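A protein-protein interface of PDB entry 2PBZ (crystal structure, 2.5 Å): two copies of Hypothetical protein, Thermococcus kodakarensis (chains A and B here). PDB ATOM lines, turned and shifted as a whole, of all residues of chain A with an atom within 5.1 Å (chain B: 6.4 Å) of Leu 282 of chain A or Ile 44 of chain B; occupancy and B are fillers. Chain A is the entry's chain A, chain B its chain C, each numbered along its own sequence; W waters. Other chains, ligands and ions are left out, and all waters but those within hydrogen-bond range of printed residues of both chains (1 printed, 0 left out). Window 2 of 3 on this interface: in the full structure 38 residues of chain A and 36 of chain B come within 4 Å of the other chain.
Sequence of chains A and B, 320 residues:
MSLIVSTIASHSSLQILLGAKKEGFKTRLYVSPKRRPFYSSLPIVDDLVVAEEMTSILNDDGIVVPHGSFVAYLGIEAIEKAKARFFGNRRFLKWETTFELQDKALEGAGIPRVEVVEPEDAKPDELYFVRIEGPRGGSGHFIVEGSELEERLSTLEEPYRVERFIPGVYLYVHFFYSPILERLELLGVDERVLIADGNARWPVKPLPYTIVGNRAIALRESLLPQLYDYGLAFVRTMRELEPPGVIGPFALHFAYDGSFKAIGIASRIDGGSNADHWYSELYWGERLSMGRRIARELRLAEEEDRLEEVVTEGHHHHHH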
ATOM      1  N   TRP A 278     -12.860  -0.034  13.830  1.00  0.00           N
ATOM      2  CA  TRP A 278     -13.383  -1.351  14.188  1.00  0.00           C
ATOM      3  C   TRP A 278     -13.471  -2.041  12.815  1.00  0.00           C
ATOM      4  O   TRP A 278     -12.425  -2.238  12.196  1.00  0.00           O
ATOM      5  CB  TRP A 278     -14.733  -1.276  14.943  1.00  0.00           C
ATOM      6  CG  TRP A 278     -15.847  -0.518  14.293  1.00  0.00           C
ATOM      7  CD1 TRP A 278     -15.956   0.833  14.174  1.00  0.00           C
ATOM      8  CD2 TRP A 278     -17.022  -1.071  13.682  1.00  0.00           C
ATOM      9  NE1 TRP A 278     -17.123   1.161  13.530  1.00  0.00           N
ATOM     10  CE2 TRP A 278     -17.799   0.012  13.213  1.00  0.00           C
ATOM     11  CE3 TRP A 278     -17.492  -2.378  13.478  1.00  0.00           C
ATOM     12  CZ2 TRP A 278     -19.025  -0.169  12.553  1.00  0.00           C
ATOM     13  CZ3 TRP A 278     -18.714  -2.559  12.819  1.00  0.00           C
ATOM     14  CH2 TRP A 278     -19.463  -1.458  12.366  1.00  0.00           C
ATOM     15  N   TYR A 279     -14.642  -2.391  12.297  1.00  0.00           N
ATOM     16  CA  TYR A 279     -14.671  -3.024  10.959  1.00  0.00           C
ATOM     17  C   TYR A 279     -13.978  -4.390  10.902  1.00  0.00           C
ATOM     18  O   TYR A 279     -14.588  -5.370  10.501  1.00  0.00           O
ATOM     19  CB  TYR A 279     -14.030  -2.109   9.907  1.00  0.00           C
ATOM     20  CG  TYR A 279     -14.913  -0.977   9.458  1.00  0.00           C
ATOM     21  CD1 TYR A 279     -16.007  -0.572  10.219  1.00  0.00           C
ATOM     22  CD2 TYR A 279     -14.625  -0.271   8.299  1.00  0.00           C
ATOM     23  CE1 TYR A 279     -16.786   0.514   9.838  1.00  0.00           C
ATOM     24  CE2 TYR A 279     -15.398   0.815   7.914  1.00  0.00           C
ATOM     25  CZ  TYR A 279     -16.475   1.207   8.685  1.00  0.00           C
ATOM     26  OH  TYR A 279     -17.217   2.300   8.324  1.00  0.00           O
ATOM     27  N   SER A 280     -12.702  -4.456  11.272  1.00  0.00           N
ATOM     28  CA  SER A 280     -11.995  -5.719  11.282  1.00  0.00           C
ATOM     29  C   SER A 280     -12.813  -6.751  12.070  1.00  0.00           C
ATOM     30  O   SER A 280     -12.686  -7.967  11.870  1.00  0.00           O
ATOM     31  CB  SER A 280     -10.633  -5.528  11.919  1.00  0.00           C
ATOM     32  OG  SER A 280     -10.725  -4.601  12.981  1.00  0.00           O
ATOM     33  N   GLU A 281     -13.649  -6.251  12.976  1.00  0.00           N
ATOM     34  CA  GLU A 281     -14.515  -7.096  13.798  1.00  0.00           C
ATOM     35  C   GLU A 281     -15.546  -7.807  12.920  1.00  0.00           C
ATOM     36  O   GLU A 281     -16.223  -8.730  13.358  1.00  0.00           O
ATOM     37  CB  GLU A 281     -15.220  -6.240  14.855  1.00  0.00           C
ATOM     38  CG  GLU A 281     -14.258  -5.639  15.853  1.00  0.00           C
ATOM     39  CD  GLU A 281     -14.901  -4.654  16.816  1.00  0.00           C
ATOM     40  OE1 GLU A 281     -14.149  -4.026  17.579  1.00  0.00           O
ATOM     41  OE2 GLU A 281     -16.141  -4.504  16.823  1.00  0.00           O
ATOM     42  N   LEU A 282     -15.667  -7.363  11.677  1.00  0.00           N
ATOM     43  CA  LEU A 282     -16.598  -7.968  10.744  1.00  0.00           C
ATOM     44  C   LEU A 282     -15.983  -9.253  10.187  1.00  0.00           C
ATOM     45  O   LEU A 282     -16.697 -10.194   9.836  1.00  0.00           O
ATOM     46  CB  LEU A 282     -16.907  -6.986   9.611  1.00  0.00           C
ATOM     47  CG  LEU A 282     -17.491  -5.638  10.050  1.00  0.00           C
ATOM     48  CD1 LEU A 282     -17.423  -4.637   8.913  1.00  0.00           C
ATOM     49  CD2 LEU A 282     -18.905  -5.834  10.530  1.00  0.00           C
ATOM     50  N   TYR A 283     -14.655  -9.299  10.116  1.00  0.00           N
ATOM     51  CA  TYR A 283     -13.975 -10.480   9.606  1.00  0.00           C
ATOM     52  C   TYR A 283     -13.456 -11.295  10.762  1.00  0.00           C
ATOM     53  O   TYR A 283     -13.254 -12.506  10.638  1.00  0.00           O
ATOM     54  CB  TYR A 283     -12.812 -10.086   8.711  1.00  0.00           C
ATOM     55  CG  TYR A 283     -13.201  -9.109   7.644  1.00  0.00           C
ATOM     56  CD1 TYR A 283     -13.187  -7.744   7.898  1.00  0.00           C
ATOM     57  CD2 TYR A 283     -13.626  -9.544   6.391  1.00  0.00           C
ATOM     58  CE1 TYR A 283     -13.586  -6.829   6.929  1.00  0.00           C
ATOM     59  CE2 TYR A 283     -14.034  -8.643   5.422  1.00  0.00           C
ATOM     60  CZ  TYR A 283     -14.012  -7.282   5.697  1.00  0.00           C
ATOM     61  OH  TYR A 283     -14.412  -6.373   4.757  1.00  0.00           O
ATOM     62  N   TRP A 284     -13.228 -10.623  11.886  1.00  0.00           N
ATOM     63  CA  TRP A 284     -12.728 -11.273  13.090  1.00  0.00           C
ATOM     64  C   TRP A 284     -13.602 -11.004  14.292  1.00  0.00           C
ATOM     65  O   TRP A 284     -14.384 -10.068  14.306  1.00  0.00           O
ATOM     66  CB  TRP A 284     -11.307 -10.820  13.364  1.00  0.00           C
ATOM     67  CG  TRP A 284     -10.355 -11.655  12.602  1.00  0.00           C
ATOM     68  CD1 TRP A 284      -9.953 -12.934  12.901  1.00  0.00           C
ATOM     69  CD2 TRP A 284      -9.728 -11.321  11.362  1.00  0.00           C
ATOM     70  NE1 TRP A 284      -9.115 -13.416  11.919  1.00  0.00           N
ATOM     71  CE2 TRP A 284      -8.959 -12.447  10.963  1.00  0.00           C
ATOM     72  CE3 TRP A 284      -9.743 -10.186  10.546  1.00  0.00           C
ATOM     73  CZ2 TRP A 284      -8.218 -12.460   9.792  1.00  0.00           C
ATOM     74  CZ3 TRP A 284      -9.016 -10.199   9.393  1.00  0.00           C
ATOM     75  CH2 TRP A 284      -8.257 -11.332   9.020  1.00  0.00           C
ATOM     76  N   SER B  13     -26.757  -2.064   9.410  1.00  0.00           N
ATOM     77  CA  SER B  13     -26.913  -3.513   9.459  1.00  0.00           C
ATOM     78  C   SER B  13     -25.628  -4.205   9.855  1.00  0.00           C
ATOM     79  O   SER B  13     -25.657  -5.306  10.381  1.00  0.00           O
ATOM     80  CB  SER B  13     -27.399  -4.059   8.114  1.00  0.00           C
ATOM     81  OG  SER B  13     -26.464  -3.810   7.085  1.00  0.00           O
ATOM     82  N   LEU B  14     -24.498  -3.559   9.611  1.00  0.00           N
ATOM     83  CA  LEU B  14     -23.206  -4.137   9.977  1.00  0.00           C
ATOM     84  C   LEU B  14     -23.112  -4.219  11.480  1.00  0.00           C
ATOM     85  O   LEU B  14     -22.824  -5.271  12.046  1.00  0.00           O
ATOM     86  CB  LEU B  14     -22.075  -3.278   9.434  1.00  0.00           C
ATOM     87  CG  LEU B  14     -22.062  -3.207   7.908  1.00  0.00           C
ATOM     88  CD1 LEU B  14     -21.060  -2.189   7.443  1.00  0.00           C
ATOM     89  CD2 LEU B  14     -21.729  -4.573   7.339  1.00  0.00           C
ATOM     90  N   GLN B  15     -23.379  -3.090  12.114  1.00  0.00           N
ATOM     91  CA  GLN B  15     -23.352  -2.977  13.555  1.00  0.00           C
ATOM     92  C   GLN B  15     -24.363  -3.957  14.133  1.00  0.00           C
ATOM     93  O   GLN B  15     -24.066  -4.716  15.054  1.00  0.00           O
ATOM     94  CB  GLN B  15     -23.733  -1.554  13.939  1.00  0.00           C
ATOM     95  CG  GLN B  15     -23.641  -1.234  15.391  1.00  0.00           C
ATOM     96  CD  GLN B  15     -24.416   0.012  15.745  1.00  0.00           C
ATOM     97  OE1 GLN B  15     -24.738   0.823  14.881  1.00  0.00           O
ATOM     98  NE2 GLN B  15     -24.712   0.176  17.024  1.00  0.00           N
ATOM     99  N   LEU B  17     -25.827  -6.752  12.803  1.00  0.00           N
ATOM    100  CA  LEU B  17     -25.495  -8.166  12.622  1.00  0.00           C
ATOM    101  C   LEU B  17     -24.299  -8.625  13.444  1.00  0.00           C
ATOM    102  O   LEU B  17     -24.316  -9.719  14.008  1.00  0.00           O
ATOM    103  CB  LEU B  17     -25.257  -8.480  11.139  1.00  0.00           C
ATOM    104  CG  LEU B  17     -26.449  -8.277  10.192  1.00  0.00           C
ATOM    105  CD1 LEU B  17     -26.095  -8.799   8.816  1.00  0.00           C
ATOM    106  CD2 LEU B  17     -27.689  -9.000  10.720  1.00  0.00           C
ATOM    107  N   LEU B  18     -23.261  -7.795  13.509  1.00  0.00           N
ATOM    108  CA  LEU B  18     -22.077  -8.145  14.287  1.00  0.00           C
ATOM    109  C   LEU B  18     -22.490  -8.304  15.747  1.00  0.00           C
ATOM    110  O   LEU B  18     -22.077  -9.244  16.407  1.00  0.00           O
ATOM    111  CB  LEU B  18     -20.989  -7.064  14.144  1.00  0.00           C
ATOM    112  CG  LEU B  18     -19.739  -7.127  15.043  1.00  0.00           C
ATOM    113  CD1 LEU B  18     -19.049  -8.467  14.912  1.00  0.00           C
ATOM    114  CD2 LEU B  18     -18.781  -6.018  14.672  1.00  0.00           C
ATOM    115  N   LYS B  21     -24.461 -11.653  16.084  1.00  0.00           N
ATOM    116  CA  LYS B  21     -23.563 -12.793  16.000  1.00  0.00           C
ATOM    117  C   LYS B  21     -22.708 -12.823  17.271  1.00  0.00           C
ATOM    118  O   LYS B  21     -22.233 -13.870  17.694  1.00  0.00           O
ATOM    119  CB  LYS B  21     -22.675 -12.676  14.750  1.00  0.00           C
ATOM    120  CG  LYS B  21     -21.539 -13.713  14.661  1.00  0.00           C
ATOM    121  CD  LYS B  21     -20.319 -13.162  13.886  1.00  0.00           C
ATOM    122  CE  LYS B  21     -19.009 -13.920  14.193  1.00  0.00           C
ATOM    123  NZ  LYS B  21     -17.790 -13.289  13.559  1.00  0.00           N
ATOM    124  N   LYS B  26     -28.281 -16.081  15.403  1.00  0.00           N
ATOM    125  CA  LYS B  26     -28.004 -16.438  14.027  1.00  0.00           C
ATOM    126  C   LYS B  26     -28.288 -15.183  13.227  1.00  0.00           C
ATOM    127  O   LYS B  26     -29.072 -14.337  13.654  1.00  0.00           O
ATOM    128  CB  LYS B  26     -28.922 -17.581  13.578  1.00  0.00           C
ATOM    129  CG  LYS B  26     -28.175 -18.707  12.874  1.00  0.00           C
ATOM    130  CD  LYS B  26     -27.090 -19.268  13.789  1.00  0.00           C
ATOM    131  CE  LYS B  26     -26.234 -20.316  13.090  1.00  0.00           C
ATOM    132  NZ  LYS B  26     -25.108 -20.788  13.951  1.00  0.00           N
ATOM    133  N   THR B  27     -27.687 -15.085  12.050  1.00  0.00           N
ATOM    134  CA  THR B  27     -27.817 -13.902  11.211  1.00  0.00           C
ATOM    135  C   THR B  27     -28.402 -14.083   9.805  1.00  0.00           C
ATOM    136  O   THR B  27     -28.031 -15.021   9.077  1.00  0.00           O
ATOM    137  CB  THR B  27     -26.418 -13.233  11.086  1.00  0.00           C
ATOM    138  OG1 THR B  27     -26.090 -12.592  12.325  1.00  0.00           O
ATOM    139  CG2 THR B  27     -26.383 -12.232   9.953  1.00  0.00           C
ATOM    140  N   ARG B  28     -29.304 -13.165   9.435  1.00  0.00           N
ATOM    141  CA  ARG B  28     -29.920 -13.147   8.107  1.00  0.00           C
ATOM    142  C   ARG B  28     -30.009 -11.730   7.566  1.00  0.00           C
ATOM    143  O   ARG B  28     -30.629 -10.859   8.171  1.00  0.00           O
ATOM    144  CB  ARG B  28     -31.325 -13.738   8.113  1.00  0.00           C
ATOM    145  CG  ARG B  28     -32.057 -13.478   6.793  1.00  0.00           C
ATOM    146  CD  ARG B  28     -33.467 -14.026   6.833  1.00  0.00           C
ATOM    147  NE  ARG B  28     -33.477 -15.468   7.040  1.00  0.00           N
ATOM    148  CZ  ARG B  28     -34.482 -16.126   7.603  1.00  0.00           C
ATOM    149  NH1 ARG B  28     -35.557 -15.465   8.020  1.00  0.00           N
ATOM    150  NH2 ARG B  28     -34.412 -17.447   7.746  1.00  0.00           N
ATOM    151  N   PHE B  38     -20.093  -7.005  -1.458  1.00  0.00           N
ATOM    152  CA  PHE B  38     -19.489  -6.559  -0.221  1.00  0.00           C
ATOM    153  C   PHE B  38     -19.967  -7.322   0.997  1.00  0.00           C
ATOM    154  O   PHE B  38     -19.153  -7.820   1.773  1.00  0.00           O
ATOM    155  CB  PHE B  38     -19.780  -5.076  -0.021  1.00  0.00           C
ATOM    156  CG  PHE B  38     -19.384  -4.569   1.323  1.00  0.00           C
ATOM    157  CD1 PHE B  38     -18.047  -4.536   1.694  1.00  0.00           C
ATOM    158  CD2 PHE B  38     -20.351  -4.188   2.246  1.00  0.00           C
ATOM    159  CE1 PHE B  38     -17.675  -4.135   2.980  1.00  0.00           C
ATOM    160  CE2 PHE B  38     -19.997  -3.789   3.525  1.00  0.00           C
ATOM    161  CZ  PHE B  38     -18.654  -3.763   3.899  1.00  0.00           C
ATOM    162  N   TYR B  39     -21.284  -7.407   1.165  1.00  0.00           N
ATOM    163  CA  TYR B  39     -21.855  -8.084   2.321  1.00  0.00           C
ATOM    164  C   TYR B  39     -21.682  -9.595   2.357  1.00  0.00           C
ATOM    165  O   TYR B  39     -21.704 -10.188   3.432  1.00  0.00           O
ATOM    166  CB  TYR B  39     -23.340  -7.761   2.456  1.00  0.00           C
ATOM    167  CG  TYR B  39     -23.640  -6.318   2.758  1.00  0.00           C
ATOM    168  CD1 TYR B  39     -23.889  -5.412   1.731  1.00  0.00           C
ATOM    169  CD2 TYR B  39     -23.688  -5.853   4.078  1.00  0.00           C
ATOM    170  CE1 TYR B  39     -24.182  -4.068   2.004  1.00  0.00           C
ATOM    171  CE2 TYR B  39     -23.988  -4.504   4.367  1.00  0.00           C
ATOM    172  CZ  TYR B  39     -24.232  -3.620   3.325  1.00  0.00           C
ATOM    173  OH  TYR B  39     -24.533  -2.300   3.589  1.00  0.00           O
ATOM    174  N   SER B  41     -19.040 -11.134   1.543  1.00  0.00           N
ATOM    175  CA  SER B  41     -17.663 -11.387   1.945  1.00  0.00           C
ATOM    176  C   SER B  41     -17.484 -11.216   3.456  1.00  0.00           C
ATOM    177  O   SER B  41     -16.384 -11.408   3.979  1.00  0.00           O
ATOM    178  CB  SER B  41     -16.719 -10.434   1.218  1.00  0.00           C
ATOM    179  OG  SER B  41     -16.821  -9.126   1.748  1.00  0.00           O
ATOM    180  N   LEU B  42     -18.563 -10.871   4.152  1.00  0.00           N
ATOM    181  CA  LEU B  42     -18.520 -10.664   5.590  1.00  0.00           C
ATOM    182  C   LEU B  42     -18.902 -11.898   6.394  1.00  0.00           C
ATOM    183  O   LEU B  42     -20.000 -12.425   6.257  1.00  0.00           O
ATOM    184  CB  LEU B  42     -19.442  -9.501   5.976  1.00  0.00           C
ATOM    185  CG  LEU B  42     -19.194  -8.201   5.214  1.00  0.00           C
ATOM    186  CD1 LEU B  42     -20.209  -7.171   5.603  1.00  0.00           C
ATOM    187  CD2 LEU B  42     -17.784  -7.707   5.499  1.00  0.00           C
ATOM    188  N   PRO B  43     -17.995 -12.366   7.263  1.00  0.00           N
ATOM    189  CA  PRO B  43     -18.215 -13.542   8.108  1.00  0.00           C
ATOM    190  C   PRO B  43     -19.331 -13.385   9.132  1.00  0.00           C
ATOM    191  O   PRO B  43     -19.599 -14.309   9.886  1.00  0.00           O
ATOM    192  CB  PRO B  43     -16.863 -13.738   8.789  1.00  0.00           C
ATOM    193  CG  PRO B  43     -15.901 -13.189   7.801  1.00  0.00           C
ATOM    194  CD  PRO B  43     -16.584 -11.945   7.307  1.00  0.00           C
ATOM    195  N   ILE B  44     -19.980 -12.227   9.179  1.00  0.00           N
ATOM    196  CA  ILE B  44     -21.035 -12.030  10.172  1.00  0.00           C
ATOM    197  C   ILE B  44     -22.436 -12.376   9.687  1.00  0.00           C
ATOM    198  O   ILE B  44     -23.389 -12.347  10.471  1.00  0.00           O
ATOM    199  CB  ILE B  44     -21.044 -10.585  10.695  1.00  0.00           C
ATOM    200  CG1 ILE B  44     -21.210  -9.608   9.524  1.00  0.00           C
ATOM    201  CG2 ILE B  44     -19.763 -10.312  11.471  1.00  0.00           C
ATOM    202  CD1 ILE B  44     -21.599  -8.193   9.934  1.00  0.00           C
ATOM    203  N   VAL B  45     -22.562 -12.705   8.402  1.00  0.00           N
ATOM    204  CA  VAL B  45     -23.868 -13.055   7.828  1.00  0.00           C
ATOM    205  C   VAL B  45     -24.024 -14.556   7.561  1.00  0.00           C
ATOM    206  O   VAL B  45     -23.233 -15.162   6.846  1.00  0.00           O
ATOM    207  CB  VAL B  45     -24.106 -12.320   6.502  1.00  0.00           C
ATOM    208  CG1 VAL B  45     -25.541 -12.543   6.039  1.00  0.00           C
ATOM    209  CG2 VAL B  45     -23.807 -10.841   6.670  1.00  0.00           C
ATOM    210  N   ASP B  46     -25.055 -15.152   8.134  1.00  0.00           N
ATOM    211  CA  ASP B  46     -25.280 -16.573   7.933  1.00  0.00           C
ATOM    212  C   ASP B  46     -26.198 -16.799   6.710  1.00  0.00           C
ATOM    213  O   ASP B  46     -25.787 -17.415   5.708  1.00  0.00           O
ATOM    214  CB  ASP B  46     -25.872 -17.203   9.204  1.00  0.00           C
ATOM    215  CG  ASP B  46     -25.008 -16.945  10.446  1.00  0.00           C
ATOM    216  OD1 ASP B  46     -23.766 -16.873  10.308  1.00  0.00           O
ATOM    217  OD2 ASP B  46     -25.563 -16.822  11.556  1.00  0.00           O
HETATM  218  O   HOH W   1     -15.028  -7.169   2.206  1.00  0.00           O
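Printed residues of chain B within 4 Å of Trp 278 of chain A: Leu 18 (3.9 Å). Of the printed residues of chain B, Glu 281 of chain A touches Leu 18. Of chain B, only Pro 43 and Ile 44 come within 4 Å of Leu 282 of chain A. Printed residues of chain A within 4 Å of Leu 18 of chain B: Trp 278 (3.9 Å) and Glu 281 (3.2 Å). Printed residues of chain A within 4 Å of Ser 41 of chain B: Tyr 283. Ile 44 of chain B touches just one residue of chain A: Leu 282. Val 45 of chain B touches none of the printed residues of chain A. The nearest residue of chain A that does not touch Ile 44 of chain B is Glu 281 of chain A (4.3 Å). The nearest printed residue of chain B that does not touch Tyr 283 of chain A is Phe 38 of chain B (4.3 Å).
The backbone carbonyl oxygen (O) of Phe 38 of chain B lies within hydrogen-bond range of the side-chain hydroxyl (OG) of Ser 41 of chain B (2.7 Å). The backbone carbonyl oxygen (O) of Trp 278 of chain A lies within hydrogen-bond range of the side-chain hydroxyl (OG) of Ser 280 of chain A. The side-chain hydroxyl (OG1) of Thr 27 of chain B lies close to the backbone carbonyl oxygen (O) of Ile 44 of chain B.
Water W1 lies within hydrogen-bond range of the side-chain hydroxyl of Ser 41 of chain B (2.7 Å) and the side-chain hydroxyl of Tyr 283 of chain A (2.7 Å).
No position is printed for both chains.
Of the 17 printed residues of chain B, 5 touch a printed residue of chain A. Hydrophobic or aromatic side chains of chain B that line the printed part of chain A: Leu 18, Leu 42, Pro 43 and Ile 44. Of the 7 printed residues of chain A, 4 touch a printed residue of chain B. Hydrophobic or aromatic side chains of chain A that line the printed part of chain B: Trp 278, Leu 282 and Tyr 283. Among the printed residues, 7 pairs touch across the chains.
Trp 278 of chain A touches Leu 18 of chain B. Glu 281 of chain A touches Leu 18 of chain B (O to CD1, 3.2 Å). Pro 43 of chain B touches Leu 282 of chain A. O of Leu 282 of chain A touches CG2 of Ile 44 of chain B, at 3.5 Å. Ser 41 of chain B touches Tyr 283 of chain A (O to CE2, 3.9 Å). Tyr 283 of chain A touches Leu 42 of chain B. CA of Tyr 283 of chain A touches CD of Pro 43 of chain B, 3.8 Å away.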
